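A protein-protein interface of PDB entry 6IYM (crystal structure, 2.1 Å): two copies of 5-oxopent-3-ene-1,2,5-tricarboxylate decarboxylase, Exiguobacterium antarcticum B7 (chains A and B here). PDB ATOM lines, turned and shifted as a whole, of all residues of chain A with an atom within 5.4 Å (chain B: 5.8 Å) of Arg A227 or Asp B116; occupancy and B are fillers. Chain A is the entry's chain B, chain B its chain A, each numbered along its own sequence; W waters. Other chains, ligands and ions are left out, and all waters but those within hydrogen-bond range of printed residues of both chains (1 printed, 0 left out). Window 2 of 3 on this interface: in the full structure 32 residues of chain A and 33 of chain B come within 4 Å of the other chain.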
ATOM      1  N   ASP A 137      -2.954 -18.223 -15.476  1.00  0.00           N
ATOM      2  CA  ASP A 137      -3.896 -18.992 -16.339  1.00  0.00           C
ATOM      3  C   ASP A 137      -4.120 -20.377 -15.709  1.00  0.00           C
ATOM      4  O   ASP A 137      -4.118 -21.400 -16.453  1.00  0.00           O
ATOM      5  CB  ASP A 137      -3.365 -19.061 -17.778  1.00  0.00           C
ATOM      6  CG  ASP A 137      -3.008 -17.691 -18.346  1.00  0.00           C
ATOM      7  OD1 ASP A 137      -3.794 -16.732 -18.109  1.00  0.00           O
ATOM      8  OD2 ASP A 137      -1.934 -17.577 -18.985  1.00  0.00           O
ATOM      9  N   LEU A 222      -9.229 -18.799  -8.039  1.00  0.00           N
ATOM     10  CA  LEU A 222      -7.862 -19.022  -8.569  1.00  0.00           C
ATOM     11  C   LEU A 222      -7.827 -18.915 -10.100  1.00  0.00           C
ATOM     12  O   LEU A 222      -6.899 -18.232 -10.626  1.00  0.00           O
ATOM     13  CB  LEU A 222      -7.380 -20.380  -8.079  1.00  0.00           C
ATOM     14  CG  LEU A 222      -6.944 -20.372  -6.612  1.00  0.00           C
ATOM     15  CD1 LEU A 222      -6.724 -21.781  -6.088  1.00  0.00           C
ATOM     16  CD2 LEU A 222      -5.692 -19.533  -6.450  1.00  0.00           C
ATOM     17  N   THR A 223      -8.792 -19.542 -10.782  1.00  0.00           N
ATOM     18  CA  THR A 223      -8.931 -19.552 -12.274  1.00  0.00           C
ATOM     19  C   THR A 223      -9.121 -18.109 -12.783  1.00  0.00           C
ATOM     20  O   THR A 223      -8.451 -17.725 -13.739  1.00  0.00           O
ATOM     21  CB  THR A 223     -10.084 -20.481 -12.699  1.00  0.00           C
ATOM     22  OG1 THR A 223      -9.560 -21.795 -12.514  1.00  0.00           O
ATOM     23  CG2 THR A 223     -10.534 -20.312 -14.133  1.00  0.00           C
ATOM     24  N   GLU A 224      -9.995 -17.344 -12.142  1.00  0.00           N
ATOM     25  CA  GLU A 224     -10.451 -16.021 -12.629  1.00  0.00           C
ATOM     26  C   GLU A 224      -9.425 -14.933 -12.272  1.00  0.00           C
ATOM     27  O   GLU A 224      -9.233 -14.056 -13.120  1.00  0.00           O
ATOM     28  CB  GLU A 224     -11.860 -15.756 -12.114  1.00  0.00           C
ATOM     29  CG  GLU A 224     -12.892 -16.625 -12.820  1.00  0.00           C
ATOM     30  CD  GLU A 224     -14.349 -16.275 -12.562  1.00  0.00           C
ATOM     31  OE1 GLU A 224     -14.619 -15.145 -12.082  1.00  0.00           O
ATOM     32  OE2 GLU A 224     -15.214 -17.146 -12.812  1.00  0.00           O
ATOM     33  N   VAL A 225      -8.721 -15.035 -11.132  1.00  0.00           N
ATOM     34  CA  VAL A 225      -7.735 -14.008 -10.675  1.00  0.00           C
ATOM     35  C   VAL A 225      -6.467 -14.120 -11.509  1.00  0.00           C
ATOM     36  O   VAL A 225      -5.830 -13.055 -11.771  1.00  0.00           O
ATOM     37  CB  VAL A 225      -7.420 -14.114  -9.162  1.00  0.00           C
ATOM     38  CG1 VAL A 225      -6.402 -13.078  -8.707  1.00  0.00           C
ATOM     39  CG2 VAL A 225      -8.659 -13.937  -8.328  1.00  0.00           C
ATOM     40  N   SER A 226      -6.066 -15.344 -11.866  1.00  0.00           N
ATOM     41  CA  SER A 226      -4.793 -15.625 -12.584  1.00  0.00           C
ATOM     42  C   SER A 226      -4.997 -15.502 -14.092  1.00  0.00           C
ATOM     43  O   SER A 226      -4.047 -15.748 -14.823  1.00  0.00           O
ATOM     44  CB  SER A 226      -4.262 -16.984 -12.266  1.00  0.00           C
ATOM     45  OG  SER A 226      -5.199 -17.980 -12.674  1.00  0.00           O
ATOM     46  N   ARG A 227      -6.200 -15.192 -14.552  1.00  0.00           N
ATOM     47  CA  ARG A 227      -6.475 -15.053 -16.006  1.00  0.00           C
ATOM     48  C   ARG A 227      -5.693 -13.823 -16.520  1.00  0.00           C
ATOM     49  O   ARG A 227      -6.147 -12.697 -16.340  1.00  0.00           O
ATOM     50  CB  ARG A 227      -7.996 -15.036 -16.205  1.00  0.00           C
ATOM     51  CG  ARG A 227      -8.527 -15.471 -17.566  1.00  0.00           C
ATOM     52  CD  ARG A 227      -7.819 -16.646 -18.225  1.00  0.00           C
ATOM     53  NE  ARG A 227      -6.995 -16.192 -19.339  1.00  0.00           N
ATOM     54  CZ  ARG A 227      -6.542 -16.960 -20.326  1.00  0.00           C
ATOM     55  NH1 ARG A 227      -5.827 -16.418 -21.301  1.00  0.00           N
ATOM     56  NH2 ARG A 227      -6.800 -18.258 -20.342  1.00  0.00           N
ATOM     57  N   GLY A 228      -4.532 -14.043 -17.128  1.00  0.00           N
ATOM     58  CA  GLY A 228      -3.664 -12.982 -17.674  1.00  0.00           C
ATOM     59  C   GLY A 228      -2.915 -12.209 -16.596  1.00  0.00           C
ATOM     60  O   GLY A 228      -2.192 -11.261 -16.967  1.00  0.00           O
ATOM     61  N   MET A 229      -3.077 -12.564 -15.311  1.00  0.00           N
ATOM     62  CA  MET A 229      -2.278 -11.971 -14.206  1.00  0.00           C
ATOM     63  C   MET A 229      -1.503 -13.073 -13.457  1.00  0.00           C
ATOM     64  O   MET A 229      -2.131 -14.061 -12.963  1.00  0.00           O
ATOM     65  CB  MET A 229      -3.175 -11.194 -13.244  1.00  0.00           C
ATOM     66  CG  MET A 229      -2.371 -10.360 -12.309  1.00  0.00           C
ATOM     67  SD  MET A 229      -3.321  -9.480 -11.069  1.00  0.00           S
ATOM     68  CE  MET A 229      -3.582 -10.796  -9.869  1.00  0.00           C
ATOM     69  N   HIS B 114      -3.112  -9.092 -24.724  1.00  0.00           N
ATOM     70  CA  HIS B 114      -4.229  -9.814 -24.042  1.00  0.00           C
ATOM     71  C   HIS B 114      -5.542  -9.650 -24.844  1.00  0.00           C
ATOM     72  O   HIS B 114      -6.566  -9.256 -24.250  1.00  0.00           O
ATOM     73  CB  HIS B 114      -4.391  -9.322 -22.580  1.00  0.00           C
ATOM     74  CG  HIS B 114      -3.198  -9.469 -21.679  1.00  0.00           C
ATOM     75  ND1 HIS B 114      -2.966 -10.606 -20.918  1.00  0.00           N
ATOM     76  CD2 HIS B 114      -2.232  -8.584 -21.327  1.00  0.00           C
ATOM     77  CE1 HIS B 114      -1.853 -10.448 -20.225  1.00  0.00           C
ATOM     78  NE2 HIS B 114      -1.383  -9.199 -20.448  1.00  0.00           N
ATOM     79  N   ALA B 115      -5.560  -9.935 -26.157  1.00  0.00           N
ATOM     80  CA  ALA B 115      -6.767  -9.722 -27.005  1.00  0.00           C
ATOM     81  C   ALA B 115      -7.954 -10.564 -26.505  1.00  0.00           C
ATOM     82  O   ALA B 115      -9.111 -10.068 -26.579  1.00  0.00           O
ATOM     83  CB  ALA B 115      -6.456  -9.982 -28.466  1.00  0.00           C
ATOM     84  N   ASP B 116      -7.716 -11.765 -25.962  1.00  0.00           N
ATOM     85  CA  ASP B 116      -8.789 -12.591 -25.321  1.00  0.00           C
ATOM     86  C   ASP B 116      -9.460 -11.842 -24.158  1.00  0.00           C
ATOM     87  O   ASP B 116     -10.667 -12.083 -23.909  1.00  0.00           O
ATOM     88  CB  ASP B 116      -8.275 -13.946 -24.820  1.00  0.00           C
ATOM     89  CG  ASP B 116      -6.957 -13.907 -24.056  1.00  0.00           C
ATOM     90  OD1 ASP B 116      -6.412 -12.788 -23.847  1.00  0.00           O
ATOM     91  OD2 ASP B 116      -6.477 -15.001 -23.674  1.00  0.00           O
ATOM     92  N   LEU B 117      -8.748 -10.970 -23.433  1.00  0.00           N
ATOM     93  CA  LEU B 117      -9.320 -10.375 -22.186  1.00  0.00           C
ATOM     94  C   LEU B 117      -9.845  -8.967 -22.433  1.00  0.00           C
ATOM     95  O   LEU B 117     -10.756  -8.584 -21.678  1.00  0.00           O
ATOM     96  CB  LEU B 117      -8.268 -10.395 -21.069  1.00  0.00           C
ATOM     97  CG  LEU B 117      -7.572 -11.742 -20.862  1.00  0.00           C
ATOM     98  CD1 LEU B 117      -6.705 -11.743 -19.609  1.00  0.00           C
ATOM     99  CD2 LEU B 117      -8.585 -12.877 -20.778  1.00  0.00           C
ATOM    100  N   THR B 118      -9.282  -8.228 -23.405  1.00  0.00           N
ATOM    101  CA  THR B 118      -9.575  -6.787 -23.639  1.00  0.00           C
ATOM    102  C   THR B 118      -9.755  -6.483 -25.132  1.00  0.00           C
ATOM    103  O   THR B 118      -8.941  -7.000 -25.933  1.00  0.00           O
ATOM    104  CB  THR B 118      -8.433  -5.836 -23.234  1.00  0.00           C
ATOM    105  OG1 THR B 118      -7.552  -6.405 -22.272  1.00  0.00           O
ATOM    106  CG2 THR B 118      -8.986  -4.536 -22.702  1.00  0.00           C
ATOM    107  N   GLN B 119     -10.731  -5.632 -25.470  1.00  0.00           N
ATOM    108  CA  GLN B 119     -10.769  -4.915 -26.777  1.00  0.00           C
ATOM    109  C   GLN B 119     -10.847  -3.403 -26.532  1.00  0.00           C
ATOM    110  O   GLN B 119     -11.165  -2.694 -27.479  1.00  0.00           O
ATOM    111  CB  GLN B 119     -11.930  -5.401 -27.654  1.00  0.00           C
ATOM    112  CG  GLN B 119     -11.864  -6.882 -28.011  1.00  0.00           C
ATOM    113  CD  GLN B 119     -10.704  -7.240 -28.903  1.00  0.00           C
ATOM    114  OE1 GLN B 119      -9.965  -8.197 -28.650  1.00  0.00           O
ATOM    115  NE2 GLN B 119     -10.543  -6.481 -29.972  1.00  0.00           N
ATOM    116  N   ARG B 170      -7.957  -5.108 -11.308  1.00  0.00           N
ATOM    117  CA  ARG B 170      -7.731  -6.182 -12.304  1.00  0.00           C
ATOM    118  C   ARG B 170      -7.423  -5.558 -13.674  1.00  0.00           C
ATOM    119  O   ARG B 170      -6.430  -5.951 -14.260  1.00  0.00           O
ATOM    120  CB  ARG B 170      -8.914  -7.152 -12.404  1.00  0.00           C
ATOM    121  CG  ARG B 170      -8.660  -8.261 -13.415  1.00  0.00           C
ATOM    122  CD  ARG B 170      -9.433  -9.556 -13.195  1.00  0.00           C
ATOM    123  NE  ARG B 170      -9.453 -10.293 -14.452  1.00  0.00           N
ATOM    124  CZ  ARG B 170      -8.435 -10.975 -14.941  1.00  0.00           C
ATOM    125  NH1 ARG B 170      -7.285 -11.062 -14.291  1.00  0.00           N
ATOM    126  NH2 ARG B 170      -8.562 -11.576 -16.105  1.00  0.00           N
ATOM    127  N   LEU B 174      -3.008  -6.620 -15.377  1.00  0.00           N
ATOM    128  CA  LEU B 174      -2.598  -7.725 -16.290  1.00  0.00           C
ATOM    129  C   LEU B 174      -1.106  -7.616 -16.568  1.00  0.00           C
ATOM    130  O   LEU B 174      -0.633  -6.470 -16.641  1.00  0.00           O
ATOM    131  CB  LEU B 174      -3.379  -7.615 -17.605  1.00  0.00           C
ATOM    132  CG  LEU B 174      -4.886  -7.822 -17.506  1.00  0.00           C
ATOM    133  CD1 LEU B 174      -5.474  -8.137 -18.872  1.00  0.00           C
ATOM    134  CD2 LEU B 174      -5.235  -8.935 -16.530  1.00  0.00           C
HETATM  135  O   HOH W   1      -6.545 -10.383 -11.799  1.00  0.00           O
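OD2 of Asp B116 is in salt-bridge range of NH1 of Arg A227, at 2.8 Å. NH2 of Arg B170 is in hydrogen-bond range of O of Arg A227 (2.7 Å).
The side-chain carboxylate (OD1) of Asp A137 lies within hydrogen-bond range of the backbone NH (N) of Gly A228 (3.0 Å). NE of Arg A227 lies within salt-bridge range of OD1 of Asp A137 (3.5 Å).
O of Glu A224 touches CZ of Arg B170 (3.7 Å). Arg B170 touches Val A225. Leu B117 touches Arg A227 (CD1 to O, 3.5 Å). O of Arg A227 touches CD2 of Leu B174 (3.9 Å). CE1 of His B114 touches O of Gly A228, 3.4 Å away. Leu B117 touches Gly A228. CA of Leu B174 touches O of Gly A228, 3.6 Å away.
Arg A227 touches four residues of chain B. Asp B116 touches just one residue of chain A: Arg A227. Printed residues of chain A within 4 Å of Leu B174: Arg A227 (3.9 Å) and Gly A228 (3.6 Å). Printed residues of chain B within 4 Å of Gly A228: His B114 (3.4 Å), Leu B117 (3.8 Å) and Leu B174 (3.6 Å). Printed residues of chain A within 4 Å of Arg B170: Glu A224 (3.7 Å), Val A225 (3.5 Å) and Arg A227 (2.7 Å). Of the printed residues of chain B, Glu A224 touches Arg B170 (3.7 Å). Of the printed residues of chain A, His B114 touches Gly A228. The nearest printed residue of chain B that does not touch Arg A227 is His B114 (6.0 Å). The nearest printed residue of chain A that does not touch Asp B116 is Asp A137 (6.4 Å).
Of the 9 printed residues of chain A, 4 touch a printed residue of chain B. Along chain A the printed residues that touch a printed residue of chain B span positions 224 to 228. Of the 8 printed residues of chain B, 5 touch a printed residue of chain A. Hydrophobic or aromatic side chains of chain B that line the printed part of chain A: His B114, Leu B117 and Leu B174. Among the printed residues, 9 pairs touch across the chains.
No position is printed for both chains.
Water W1 lies within hydrogen-bond range of NH1 of Arg B170 (2.7 Å), O of Val A225 (2.8 Å) and SD of Met A229 (3.4 Å).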
